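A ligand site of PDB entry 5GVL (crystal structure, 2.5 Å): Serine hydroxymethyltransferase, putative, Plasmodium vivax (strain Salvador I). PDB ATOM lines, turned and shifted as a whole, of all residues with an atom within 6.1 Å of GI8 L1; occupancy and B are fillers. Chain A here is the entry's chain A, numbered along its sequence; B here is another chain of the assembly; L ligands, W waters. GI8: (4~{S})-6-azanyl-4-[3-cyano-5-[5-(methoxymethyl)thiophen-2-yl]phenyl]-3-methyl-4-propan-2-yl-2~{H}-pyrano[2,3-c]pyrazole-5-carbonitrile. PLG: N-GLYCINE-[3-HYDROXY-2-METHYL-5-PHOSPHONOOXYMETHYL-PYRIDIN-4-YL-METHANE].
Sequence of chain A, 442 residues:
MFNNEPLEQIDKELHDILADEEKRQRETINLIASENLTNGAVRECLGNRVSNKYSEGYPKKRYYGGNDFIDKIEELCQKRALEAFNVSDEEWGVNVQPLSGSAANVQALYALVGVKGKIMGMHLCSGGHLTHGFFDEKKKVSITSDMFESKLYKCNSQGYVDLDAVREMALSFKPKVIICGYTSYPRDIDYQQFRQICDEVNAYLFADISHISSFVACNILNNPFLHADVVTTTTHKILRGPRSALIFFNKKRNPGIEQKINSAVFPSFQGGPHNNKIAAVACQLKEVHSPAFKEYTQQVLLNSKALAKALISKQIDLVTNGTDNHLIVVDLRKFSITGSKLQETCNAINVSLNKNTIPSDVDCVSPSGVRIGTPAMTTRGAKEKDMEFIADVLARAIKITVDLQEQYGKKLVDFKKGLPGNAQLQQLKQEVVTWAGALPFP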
ATOM      1  N   HIS A 123     -32.748  -6.298 -13.377  1.00  0.00           N
ATOM      2  CA  HIS A 123     -31.509  -5.648 -12.949  1.00  0.00           C
ATOM      3  C   HIS A 123     -31.508  -5.470 -11.444  1.00  0.00           C
ATOM      4  O   HIS A 123     -32.560  -5.261 -10.834  1.00  0.00           O
ATOM      5  CB  HIS A 123     -31.398  -4.288 -13.643  1.00  0.00           C
ATOM      6  CG  HIS A 123     -30.025  -3.690 -13.619  1.00  0.00           C
ATOM      7  ND1 HIS A 123     -29.519  -3.016 -12.520  1.00  0.00           N
ATOM      8  CD2 HIS A 123     -29.055  -3.646 -14.562  1.00  0.00           C
ATOM      9  CE1 HIS A 123     -28.296  -2.599 -12.790  1.00  0.00           C
ATOM     10  NE2 HIS A 123     -27.995  -2.962 -14.016  1.00  0.00           N
ATOM     11  N   LEU A 124     -30.310  -5.564 -10.844  1.00  0.00           N
ATOM     12  CA  LEU A 124     -30.126  -5.378  -9.400  1.00  0.00           C
ATOM     13  C   LEU A 124     -30.656  -4.041  -8.894  1.00  0.00           C
ATOM     14  O   LEU A 124     -31.337  -4.015  -7.866  1.00  0.00           O
ATOM     15  CB  LEU A 124     -28.652  -5.520  -9.041  1.00  0.00           C
ATOM     16  CG  LEU A 124     -28.240  -5.508  -7.569  1.00  0.00           C
ATOM     17  CD1 LEU A 124     -28.085  -6.930  -7.045  1.00  0.00           C
ATOM     18  CD2 LEU A 124     -26.936  -4.733  -7.409  1.00  0.00           C
ATOM     19  N   CYS A 125     -30.324  -2.957  -9.608  1.00  0.00           N
ATOM     20  CA  CYS A 125     -30.801  -1.584  -9.298  1.00  0.00           C
ATOM     21  C   CYS A 125     -32.329  -1.440  -9.398  1.00  0.00           C
ATOM     22  O   CYS A 125     -32.916  -0.585  -8.739  1.00  0.00           O
ATOM     23  CB  CYS A 125     -30.115  -0.529 -10.171  1.00  0.00           C
ATOM     24  SG  CYS A 125     -28.360  -0.218  -9.833  1.00  0.00           S
ATOM     25  N   SER A 126     -32.949  -2.282 -10.210  1.00  0.00           N
ATOM     26  CA  SER A 126     -34.388  -2.311 -10.380  1.00  0.00           C
ATOM     27  C   SER A 126     -35.132  -3.193  -9.364  1.00  0.00           C
ATOM     28  O   SER A 126     -36.359  -3.122  -9.285  1.00  0.00           O
ATOM     29  CB  SER A 126     -34.741  -2.758 -11.801  1.00  0.00           C
ATOM     30  OG  SER A 126     -34.516  -1.704 -12.718  1.00  0.00           O
ATOM     31  N   GLY A 127     -34.395  -4.017  -8.607  1.00  0.00           N
ATOM     32  CA  GLY A 127     -35.005  -4.860  -7.563  1.00  0.00           C
ATOM     33  C   GLY A 127     -34.751  -6.344  -7.685  1.00  0.00           C
ATOM     34  O   GLY A 127     -35.198  -7.127  -6.839  1.00  0.00           O
ATOM     35  N   GLY A 128     -34.009  -6.724  -8.718  1.00  0.00           N
ATOM     36  CA  GLY A 128     -33.669  -8.124  -8.978  1.00  0.00           C
ATOM     37  C   GLY A 128     -32.481  -8.657  -8.203  1.00  0.00           C
ATOM     38  O   GLY A 128     -31.700  -7.879  -7.644  1.00  0.00           O
ATOM     39  N   HIS A 129     -32.356  -9.990  -8.156  1.00  0.00           N
ATOM     40  CA  HIS A 129     -31.275 -10.616  -7.413  1.00  0.00           C
ATOM     41  C   HIS A 129     -29.960 -10.688  -8.189  1.00  0.00           C
ATOM     42  O   HIS A 129     -29.945 -10.568  -9.415  1.00  0.00           O
ATOM     43  CB  HIS A 129     -31.641 -11.991  -6.845  1.00  0.00           C
ATOM     44  CG  HIS A 129     -30.761 -12.395  -5.698  1.00  0.00           C
ATOM     45  ND1 HIS A 129     -29.772 -13.348  -5.833  1.00  0.00           N
ATOM     46  CD2 HIS A 129     -30.660 -11.927  -4.439  1.00  0.00           C
ATOM     47  CE1 HIS A 129     -29.135 -13.480  -4.687  1.00  0.00           C
ATOM     48  NE2 HIS A 129     -29.645 -12.626  -3.826  1.00  0.00           N
ATOM     49  N   LEU A 130     -28.864 -10.841  -7.452  1.00  0.00           N
ATOM     50  CA  LEU A 130     -27.563 -11.138  -8.027  1.00  0.00           C
ATOM     51  C   LEU A 130     -27.633 -12.356  -8.948  1.00  0.00           C
ATOM     52  O   LEU A 130     -27.156 -12.305 -10.079  1.00  0.00           O
ATOM     53  CB  LEU A 130     -26.524 -11.382  -6.924  1.00  0.00           C
ATOM     54  CG  LEU A 130     -26.074 -10.218  -6.019  1.00  0.00           C
ATOM     55  CD1 LEU A 130     -25.361 -10.761  -4.807  1.00  0.00           C
ATOM     56  CD2 LEU A 130     -25.184  -9.228  -6.753  1.00  0.00           C
ATOM     57  N   PHE A 134     -26.970 -10.894 -13.007  1.00  0.00           N
ATOM     58  CA  PHE A 134     -26.431  -9.563 -12.808  1.00  0.00           C
ATOM     59  C   PHE A 134     -24.949  -9.411 -13.147  1.00  0.00           C
ATOM     60  O   PHE A 134     -24.103 -10.190 -12.690  1.00  0.00           O
ATOM     61  CB  PHE A 134     -26.695  -9.047 -11.392  1.00  0.00           C
ATOM     62  CG  PHE A 134     -26.094  -7.697 -11.140  1.00  0.00           C
ATOM     63  CD1 PHE A 134     -26.670  -6.547 -11.689  1.00  0.00           C
ATOM     64  CD2 PHE A 134     -24.928  -7.568 -10.404  1.00  0.00           C
ATOM     65  CE1 PHE A 134     -26.094  -5.299 -11.487  1.00  0.00           C
ATOM     66  CE2 PHE A 134     -24.341  -6.324 -10.195  1.00  0.00           C
ATOM     67  CZ  PHE A 134     -24.935  -5.185 -10.737  1.00  0.00           C
ATOM     68  N   ASP A 136     -22.007  -5.935 -14.134  1.00  0.00           N
ATOM     69  CA  ASP A 136     -21.635  -4.534 -14.213  1.00  0.00           C
ATOM     70  C   ASP A 136     -20.928  -4.333 -15.547  1.00  0.00           C
ATOM     71  O   ASP A 136     -20.424  -5.286 -16.146  1.00  0.00           O
ATOM     72  CB  ASP A 136     -20.650  -4.229 -13.078  1.00  0.00           C
ATOM     73  CG  ASP A 136     -20.558  -2.773 -12.726  1.00  0.00           C
ATOM     74  OD1 ASP A 136     -21.182  -1.921 -13.407  1.00  0.00           O
ATOM     75  OD2 ASP A 136     -19.842  -2.470 -11.753  1.00  0.00           O
ATOM     76  N   VAL A 141     -20.332  -9.708 -12.246  1.00  0.00           N
ATOM     77  CA  VAL A 141     -20.443  -9.747 -10.785  1.00  0.00           C
ATOM     78  C   VAL A 141     -20.945 -11.104 -10.260  1.00  0.00           C
ATOM     79  O   VAL A 141     -20.391 -11.656  -9.318  1.00  0.00           O
ATOM     80  CB  VAL A 141     -21.315  -8.583 -10.279  1.00  0.00           C
ATOM     81  CG1 VAL A 141     -21.266  -8.480  -8.756  1.00  0.00           C
ATOM     82  CG2 VAL A 141     -20.851  -7.266 -10.891  1.00  0.00           C
ATOM     83  N   THR A 183     -35.879  -9.551  -5.273  1.00  0.00           N
ATOM     84  CA  THR A 183     -35.281  -9.283  -3.958  1.00  0.00           C
ATOM     85  C   THR A 183     -35.839  -8.028  -3.289  1.00  0.00           C
ATOM     86  O   THR A 183     -36.092  -8.039  -2.077  1.00  0.00           O
ATOM     87  CB  THR A 183     -33.732  -9.322  -3.958  1.00  0.00           C
ATOM     88  OG1 THR A 183     -33.187  -8.157  -3.318  1.00  0.00           O
ATOM     89  CG2 THR A 183     -33.214  -9.349  -5.284  1.00  0.00           C
ATOM     90  N   SER A 184     -36.032  -6.962  -4.058  1.00  0.00           N
ATOM     91  CA  SER A 184     -36.567  -5.723  -3.508  1.00  0.00           C
ATOM     92  C   SER A 184     -37.599  -5.071  -4.412  1.00  0.00           C
ATOM     93  O   SER A 184     -37.483  -3.908  -4.784  1.00  0.00           O
ATOM     94  CB  SER A 184     -35.441  -4.754  -3.112  1.00  0.00           C
ATOM     95  OG  SER A 184     -34.339  -4.800  -3.997  1.00  0.00           O
ATOM     96  N   ASN A 354     -31.454  -2.088   5.454  1.00  0.00           N
ATOM     97  CA  ASN A 354     -30.378  -2.000   4.487  1.00  0.00           C
ATOM     98  C   ASN A 354     -30.615  -0.903   3.489  1.00  0.00           C
ATOM     99  O   ASN A 354     -31.747  -0.600   3.138  1.00  0.00           O
ATOM    100  CB  ASN A 354     -30.138  -3.332   3.761  1.00  0.00           C
ATOM    101  CG  ASN A 354     -31.316  -3.761   2.894  1.00  0.00           C
ATOM    102  OD1 ASN A 354     -32.287  -4.350   3.392  1.00  0.00           O
ATOM    103  ND2 ASN A 354     -31.232  -3.470   1.591  1.00  0.00           N
ATOM    104  N   LYS A 355     -29.514  -0.323   3.033  1.00  0.00           N
ATOM    105  CA  LYS A 355     -29.534   0.575   1.907  1.00  0.00           C
ATOM    106  C   LYS A 355     -29.967  -0.190   0.665  1.00  0.00           C
ATOM    107  O   LYS A 355     -29.596  -1.340   0.480  1.00  0.00           O
ATOM    108  CB  LYS A 355     -28.154   1.215   1.712  1.00  0.00           C
ATOM    109  CG  LYS A 355     -27.002   0.216   1.657  1.00  0.00           C
ATOM    110  CD  LYS A 355     -25.753   0.799   1.031  1.00  0.00           C
ATOM    111  CE  LYS A 355     -24.817  -0.298   0.577  1.00  0.00           C
ATOM    112  NZ  LYS A 355     -23.441  -0.033   1.053  1.00  0.00           N
ATOM    113  N   ASN A 356     -30.776   0.465  -0.164  1.00  0.00           N
ATOM    114  CA  ASN A 356     -31.288  -0.112  -1.392  1.00  0.00           C
ATOM    115  C   ASN A 356     -31.257   0.902  -2.524  1.00  0.00           C
ATOM    116  O   ASN A 356     -31.424   2.114  -2.295  1.00  0.00           O
ATOM    117  CB  ASN A 356     -32.721  -0.607  -1.181  1.00  0.00           C
ATOM    118  CG  ASN A 356     -33.047  -1.796  -2.043  1.00  0.00           C
ATOM    119  OD1 ASN A 356     -32.945  -2.948  -1.597  1.00  0.00           O
ATOM    120  ND2 ASN A 356     -33.413  -1.542  -3.283  1.00  0.00           N
ATOM    121  N   THR A 357     -31.042   0.424  -3.746  1.00  0.00           N
ATOM    122  CA  THR A 357     -31.089   1.290  -4.943  1.00  0.00           C
ATOM    123  C   THR A 357     -32.517   1.712  -5.282  1.00  0.00           C
ATOM    124  O   THR A 357     -33.486   1.110  -4.834  1.00  0.00           O
ATOM    125  CB  THR A 357     -30.461   0.602  -6.162  1.00  0.00           C
ATOM    126  OG1 THR A 357     -31.095  -0.660  -6.366  1.00  0.00           O
ATOM    127  CG2 THR A 357     -28.968   0.392  -5.985  1.00  0.00           C
ATOM    128  N   ASP A 363     -25.518   4.347  -9.042  1.00  0.00           N
ATOM    129  CA  ASP A 363     -24.458   4.014  -8.099  1.00  0.00           C
ATOM    130  C   ASP A 363     -24.884   2.854  -7.190  1.00  0.00           C
ATOM    131  O   ASP A 363     -26.014   2.828  -6.708  1.00  0.00           O
ATOM    132  CB  ASP A 363     -24.106   5.255  -7.257  1.00  0.00           C
ATOM    133  CG  ASP A 363     -22.898   5.062  -6.365  1.00  0.00           C
ATOM    134  OD1 ASP A 363     -22.922   4.183  -5.490  1.00  0.00           O
ATOM    135  OD2 ASP A 363     -21.914   5.806  -6.532  1.00  0.00           O
ATOM    136  N   CYS A 364     -23.970   1.931  -6.940  1.00  0.00           N
ATOM    137  CA  CYS A 364     -24.254   0.752  -6.115  1.00  0.00           C
ATOM    138  C   CYS A 364     -23.649   0.836  -4.720  1.00  0.00           C
ATOM    139  O   CYS A 364     -24.158   0.208  -3.787  1.00  0.00           O
ATOM    140  CB  CYS A 364     -23.806  -0.539  -6.804  1.00  0.00           C
ATOM    141  SG  CYS A 364     -25.043  -1.186  -7.946  1.00  0.00           S
ATOM    142  N   VAL A 365     -22.564   1.600  -4.592  1.00  0.00           N
ATOM    143  CA  VAL A 365     -21.862   1.801  -3.320  1.00  0.00           C
ATOM    144  C   VAL A 365     -22.687   2.764  -2.427  1.00  0.00           C
ATOM    145  O   VAL A 365     -22.916   2.469  -1.244  1.00  0.00           O
ATOM    146  CB  VAL A 365     -20.391   2.274  -3.508  1.00  0.00           C
ATOM    147  CG1 VAL A 365     -19.621   2.224  -2.195  1.00  0.00           C
ATOM    148  CG2 VAL A 365     -19.680   1.433  -4.558  1.00  0.00           C
ATOM    149  N   SER A 366     -23.135   3.888  -3.018  1.00  0.00           N
ATOM    150  CA  SER A 366     -24.059   4.835  -2.356  1.00  0.00           C
ATOM    151  C   SER A 366     -25.393   4.942  -3.118  1.00  0.00           C
ATOM    152  O   SER A 366     -25.458   5.540  -4.185  1.00  0.00           O
ATOM    153  CB  SER A 366     -23.402   6.219  -2.166  1.00  0.00           C
ATOM    154  OG  SER A 366     -23.025   6.771  -3.422  1.00  0.00           O
ATOM    155  N   PRO A 367     -26.460   4.329  -2.575  1.00  0.00           N
ATOM    156  CA  PRO A 367     -27.791   4.408  -3.188  1.00  0.00           C
ATOM    157  C   PRO A 367     -28.690   5.489  -2.561  1.00  0.00           C
ATOM    158  O   PRO A 367     -28.368   6.032  -1.498  1.00  0.00           O
ATOM    159  CB  PRO A 367     -28.362   3.031  -2.913  1.00  0.00           C
ATOM    160  CG  PRO A 367     -27.792   2.675  -1.569  1.00  0.00           C
ATOM    161  CD  PRO A 367     -26.472   3.375  -1.435  1.00  0.00           C
ATOM    162  N   ARG A 371     -34.380  -0.175   2.129  1.00  0.00           N
ATOM    163  CA  ARG A 371     -35.470  -1.117   2.060  1.00  0.00           C
ATOM    164  C   ARG A 371     -35.845  -1.577   3.471  1.00  0.00           C
ATOM    165  O   ARG A 371     -34.972  -1.834   4.297  1.00  0.00           O
ATOM    166  CB  ARG A 371     -35.105  -2.292   1.153  1.00  0.00           C
ATOM    167  CG  ARG A 371     -36.238  -3.272   0.877  1.00  0.00           C
ATOM    168  CD  ARG A 371     -35.710  -4.609   0.399  1.00  0.00           C
ATOM    169  NE  ARG A 371     -34.810  -5.269   1.367  1.00  0.00           N
ATOM    170  CZ  ARG A 371     -34.159  -6.408   1.140  1.00  0.00           C
ATOM    171  NH1 ARG A 371     -34.291  -7.058  -0.011  1.00  0.00           N
ATOM    172  NH2 ARG A 371     -33.377  -6.909   2.071  1.00  0.00           N
ATOM    173  N   GLU B  56     -24.467 -10.395   4.239  1.00  0.00           N
ATOM    174  CA  GLU B  56     -23.800 -10.407   2.941  1.00  0.00           C
ATOM    175  C   GLU B  56     -22.598  -9.459   2.882  1.00  0.00           C
ATOM    176  O   GLU B  56     -22.681  -8.314   3.328  1.00  0.00           O
ATOM    177  CB  GLU B  56     -24.789 -10.083   1.839  1.00  0.00           C
ATOM    178  CG  GLU B  56     -25.213 -11.308   1.071  1.00  0.00           C
ATOM    179  CD  GLU B  56     -26.402 -11.092   0.166  1.00  0.00           C
ATOM    180  OE1 GLU B  56     -27.529 -11.114   0.683  1.00  0.00           O
ATOM    181  OE2 GLU B  56     -26.224 -10.951  -1.059  1.00  0.00           O
ATOM    182  N   TYR B  63     -23.690  -5.464   3.852  1.00  0.00           N
ATOM    183  CA  TYR B  63     -24.752  -4.789   3.124  1.00  0.00           C
ATOM    184  C   TYR B  63     -26.000  -4.658   3.994  1.00  0.00           C
ATOM    185  O   TYR B  63     -27.100  -4.437   3.497  1.00  0.00           O
ATOM    186  CB  TYR B  63     -25.053  -5.519   1.816  1.00  0.00           C
ATOM    187  CG  TYR B  63     -24.007  -5.350   0.719  1.00  0.00           C
ATOM    188  CD1 TYR B  63     -22.876  -6.160   0.674  1.00  0.00           C
ATOM    189  CD2 TYR B  63     -24.169  -4.383  -0.280  1.00  0.00           C
ATOM    190  CE1 TYR B  63     -21.922  -6.010  -0.328  1.00  0.00           C
ATOM    191  CE2 TYR B  63     -23.220  -4.224  -1.283  1.00  0.00           C
ATOM    192  CZ  TYR B  63     -22.103  -5.041  -1.300  1.00  0.00           C
ATOM    193  OH  TYR B  63     -21.155  -4.895  -2.296  1.00  0.00           O
ATOM    194  N   TYR B  64     -25.831  -4.834   5.301  1.00  0.00           N
ATOM    195  CA  TYR B  64     -26.910  -4.697   6.272  1.00  0.00           C
ATOM    196  C   TYR B  64     -26.377  -4.091   7.564  1.00  0.00           C
ATOM    197  O   TYR B  64     -25.180  -4.258   7.902  1.00  0.00           O
ATOM    198  CB  TYR B  64     -27.620  -6.043   6.567  1.00  0.00           C
ATOM    199  CG  TYR B  64     -28.007  -6.826   5.327  1.00  0.00           C
ATOM    200  CD1 TYR B  64     -29.180  -6.530   4.627  1.00  0.00           C
ATOM    201  CD2 TYR B  64     -27.182  -7.853   4.838  1.00  0.00           C
ATOM    202  CE1 TYR B  64     -29.521  -7.220   3.466  1.00  0.00           C
ATOM    203  CE2 TYR B  64     -27.519  -8.564   3.684  1.00  0.00           C
ATOM    204  CZ  TYR B  64     -28.692  -8.255   3.005  1.00  0.00           C
ATOM    205  OH  TYR B  64     -29.023  -8.950   1.866  1.00  0.00           O
ATOM    206  N   PHE B 266     -18.314 -14.623  -2.586  1.00  0.00           N
ATOM    207  CA  PHE B 266     -19.358 -13.610  -2.716  1.00  0.00           C
ATOM    208  C   PHE B 266     -18.776 -12.414  -3.462  1.00  0.00           C
ATOM    209  O   PHE B 266     -17.688 -11.996  -3.109  1.00  0.00           O
ATOM    210  CB  PHE B 266     -19.883 -13.182  -1.340  1.00  0.00           C
ATOM    211  CG  PHE B 266     -20.825 -12.005  -1.390  1.00  0.00           C
ATOM    212  CD1 PHE B 266     -22.189 -12.194  -1.696  1.00  0.00           C
ATOM    213  CD2 PHE B 266     -20.371 -10.702  -1.138  1.00  0.00           C
ATOM    214  CE1 PHE B 266     -23.065 -11.106  -1.763  1.00  0.00           C
ATOM    215  CE2 PHE B 266     -21.242  -9.622  -1.190  1.00  0.00           C
ATOM    216  CZ  PHE B 266     -22.583  -9.821  -1.495  1.00  0.00           C
ATOM    217  N   PRO B 267     -19.477 -11.840  -4.454  1.00  0.00           N
ATOM    218  CA  PRO B 267     -20.869 -12.192  -4.802  1.00  0.00           C
ATOM    219  C   PRO B 267     -21.031 -13.091  -6.029  1.00  0.00           C
ATOM    220  O   PRO B 267     -22.153 -13.252  -6.508  1.00  0.00           O
ATOM    221  CB  PRO B 267     -21.496 -10.836  -5.080  1.00  0.00           C
ATOM    222  CG  PRO B 267     -20.379 -10.038  -5.666  1.00  0.00           C
ATOM    223  CD  PRO B 267     -19.133 -10.488  -4.952  1.00  0.00           C
HETATM  224  N9  GI8 L   1     -30.838  -2.987  -3.941  1.00  0.00           N
HETATM  225  C8  GI8 L   1     -30.514  -4.096  -3.852  1.00  0.00           C
HETATM  226  C3  GI8 L   1     -30.144  -5.316  -3.738  1.00  0.00           C
HETATM  227  C2  GI8 L   1     -30.654  -6.232  -4.621  1.00  0.00           C
HETATM  228  N7  GI8 L   1     -31.517  -5.891  -5.568  1.00  0.00           N
HETATM  229  O1  GI8 L   1     -30.289  -7.637  -4.582  1.00  0.00           O
HETATM  230  C6  GI8 L   1     -29.302  -8.058  -3.741  1.00  0.00           C
HETATM  231  N12 GI8 L   1     -28.784  -9.294  -3.704  1.00  0.00           N
HETATM  232  N11 GI8 L   1     -27.828  -9.250  -2.665  1.00  0.00           N
HETATM  233  C10 GI8 L   1     -27.742  -8.037  -2.084  1.00  0.00           C
HETATM  234  C13 GI8 L   1     -26.782  -7.689  -0.965  1.00  0.00           C
HETATM  235  C5  GI8 L   1     -28.734  -7.148  -2.762  1.00  0.00           C
HETATM  236  C4  GI8 L   1     -29.135  -5.686  -2.627  1.00  0.00           C
HETATM  237  C14 GI8 L   1     -29.790  -5.423  -1.240  1.00  0.00           C
HETATM  238  C16 GI8 L   1     -28.846  -5.343  -0.033  1.00  0.00           C
HETATM  239  C15 GI8 L   1     -30.941  -6.374  -0.902  1.00  0.00           C
HETATM  240  C17 GI8 L   1     -27.914  -4.807  -2.897  1.00  0.00           C
HETATM  241  C18 GI8 L   1     -27.925  -3.453  -2.563  1.00  0.00           C
HETATM  242  C19 GI8 L   1     -26.846  -2.617  -2.812  1.00  0.00           C
HETATM  243  C23 GI8 L   1     -26.920  -1.388  -2.472  1.00  0.00           C
HETATM  244  N24 GI8 L   1     -26.975  -0.278  -2.165  1.00  0.00           N
HETATM  245  C22 GI8 L   1     -26.769  -5.290  -3.527  1.00  0.00           C
HETATM  246  C21 GI8 L   1     -25.668  -4.462  -3.774  1.00  0.00           C
HETATM  247  C20 GI8 L   1     -25.702  -3.112  -3.434  1.00  0.00           C
HETATM  248  C25 GI8 L   1     -24.499  -5.098  -4.421  1.00  0.00           C
HETATM  249  S29 GI8 L   1     -23.693  -4.233  -5.668  1.00  0.00           S
HETATM  250  C28 GI8 L   1     -22.545  -5.472  -5.961  1.00  0.00           C
HETATM  251  C27 GI8 L   1     -22.802  -6.537  -5.109  1.00  0.00           C
HETATM  252  C26 GI8 L   1     -23.884  -6.324  -4.245  1.00  0.00           C
HETATM  253  C30 GI8 L   1     -21.535  -5.207  -7.054  1.00  0.00           C
HETATM  254  O31 GI8 L   1     -20.204  -5.042  -6.572  1.00  0.00           O
HETATM  255  C32 GI8 L   1     -19.544  -6.239  -6.118  1.00  0.00           C
HETATM  256  N1  PLG L   2     -33.369 -14.937  -4.361  1.00  0.00           N
HETATM  257  C2  PLG L   2     -33.879 -13.770  -3.929  1.00  0.00           C
HETATM  258  C2A PLG L   2     -35.104 -13.197  -4.615  1.00  0.00           C
HETATM  259  C3  PLG L   2     -33.220 -13.089  -2.759  1.00  0.00           C
HETATM  260  O3  PLG L   2     -33.715 -11.922  -2.284  1.00  0.00           O
HETATM  261  C4  PLG L   2     -32.024 -13.730  -2.123  1.00  0.00           C
HETATM  262  C4A PLG L   2     -31.269 -13.095  -0.962  1.00  0.00           C
HETATM  263  C5  PLG L   2     -31.580 -15.020  -2.741  1.00  0.00           C
HETATM  264  C6  PLG L   2     -32.294 -15.530  -3.824  1.00  0.00           C
HETATM  265  C5A PLG L   2     -30.370 -15.791  -2.266  1.00  0.00           C
HETATM  266  OP4 PLG L   2     -30.517 -16.287  -0.942  1.00  0.00           O
HETATM  267  P   PLG L   2     -29.224 -16.751  -0.134  1.00  0.00           P
HETATM  268  OP1 PLG L   2     -28.250 -17.418  -1.067  1.00  0.00           O
HETATM  269  OP2 PLG L   2     -28.712 -15.422   0.389  1.00  0.00           O
HETATM  270  OP3 PLG L   2     -29.807 -17.697   0.877  1.00  0.00           O
HETATM  271  C   PLG L   2     -32.073  -9.836   0.664  1.00  0.00           C
HETATM  272  O   PLG L   2     -31.727  -9.384   1.772  1.00  0.00           O
HETATM  273  OXT PLG L   2     -33.202  -9.621   0.180  1.00  0.00           O
HETATM  274  CA  PLG L   2     -31.121 -10.701  -0.118  1.00  0.00           C
HETATM  275  N   PLG L   2     -31.874 -11.858  -0.522  1.00  0.00           N
HETATM  276  O   HOH W   1     -33.283  -3.155  -5.965  1.00  0.00           O
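A nitrogen (N11) of GI8 L1 lies within hydrogen-bond range of the side-chain carboxylate (OE2) of Glu 56 of chain B, at 2.8 Å. O of Gly 128 lies within hydrogen-bond range of N7 of GI8 L1 (2.9 Å). A nitrogen (N7) of GI8 L1 lies within hydrogen-bond range of the backbone carbonyl oxygen (O) of Leu 124 (3.0 Å). The side-chain amide nitrogen (ND2) of Asn 356 is in hydrogen-bond range of a nitrogen (N9) of GI8 L1. The side-chain hydroxyl (OG1) of Thr 183 sits at hydrogen-bond distance from an oxygen (O1) of GI8 L1 (3.2 Å). NE2 of His 129 sits close to N12 of GI8 L1. The backbone NH of Thr 357 sits at hydrogen-bond distance from a nitrogen (N9) of GI8 L1 (3.4 Å). OG1 of Thr 357 is in hydrogen-bond range of N9 of GI8 L1 (3.4 Å). The side-chain hydroxyl (OG) of Ser 184 lies within hydrogen-bond range of a nitrogen (N7) of GI8 L1, at 3.4 Å. The guanidinium group (NH1) of Arg 371 is in salt-bridge range of an oxygen (OXT) of PLG L2. O of PLG L2 sits at hydrogen-bond distance from OH of Tyr 64 of chain B, at 2.7 Å.
The side-chain carboxylate (OE1) of Glu 56 of chain B lies within hydrogen-bond range of the side-chain hydroxyl (OH) of Tyr 64 of chain B, 2.9 Å away. The backbone NH (N) of Gly 128 lies within hydrogen-bond range of the backbone carbonyl oxygen (O) of His 123. The side-chain amide oxygen of Asn 356 is in hydrogen-bond range of the side-chain hydroxyl of Ser 184 (3.3 Å). The backbone carbonyl oxygen of Thr 183 is in hydrogen-bond range of the guanidinium group of Arg 371. O of Cys 125 is in hydrogen-bond range of OG1 of Thr 357, 3.0 Å away. O of Gly 127 lies within hydrogen-bond range of N of Ser 184. The backbone carbonyl oxygen of Asn 354 is in hydrogen-bond range of the backbone NH of Arg 371, at 2.9 Å. NZ of Lys 355 sits at hydrogen-bond distance from O of Val 365, 3.4 Å away.
N24 of GI8 L1 sits close to O of Cys 364 (3.3 Å). Gly 127 touches GI8 L1. Leu 130 touches GI8 L1 (CD1 to N11, 3.6 Å). CG1 of Val 141 touches C30 of GI8 L1, at 3.7 Å. ND2 of Asn 354 touches C16 of GI8 L1, 3.4 Å away. CE of Lys 355 touches N24 of GI8 L1 (3.5 Å). Pro 367 touches GI8 L1. Arg 371 touches GI8 L1. CE2 of Tyr 63 of chain B touches C20 of GI8 L1, 3.5 Å away. Tyr 64 of chain B touches GI8 L1 (OH to C13, 3.8 Å). Pro 267 of chain B touches GI8 L1 (CG to C32, 3.9 Å). Hydrophobic or aromatic side chains within 4 Å of GI8 L1: Leu 124, His 129, Leu 130, Val 141, Pro 367, Tyr 63 of chain B and Pro 267 of chain B. Of the 28 residues printed, 19 come within 4 Å of GI8 L1. The nearest printed residue that does not touch GI8 L1 is Phe 134 (4.4 Å).
Water W1 lies within hydrogen-bond range of OG of Ser 184 (2.8 Å), O of Leu 124 (2.9 Å), N of Gly 127 (3.0 Å), ND2 of Asn 356 (3.1 Å), N9 of GI8 L1 (3.2 Å) and OG1 of Thr 357 (3.3 Å).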
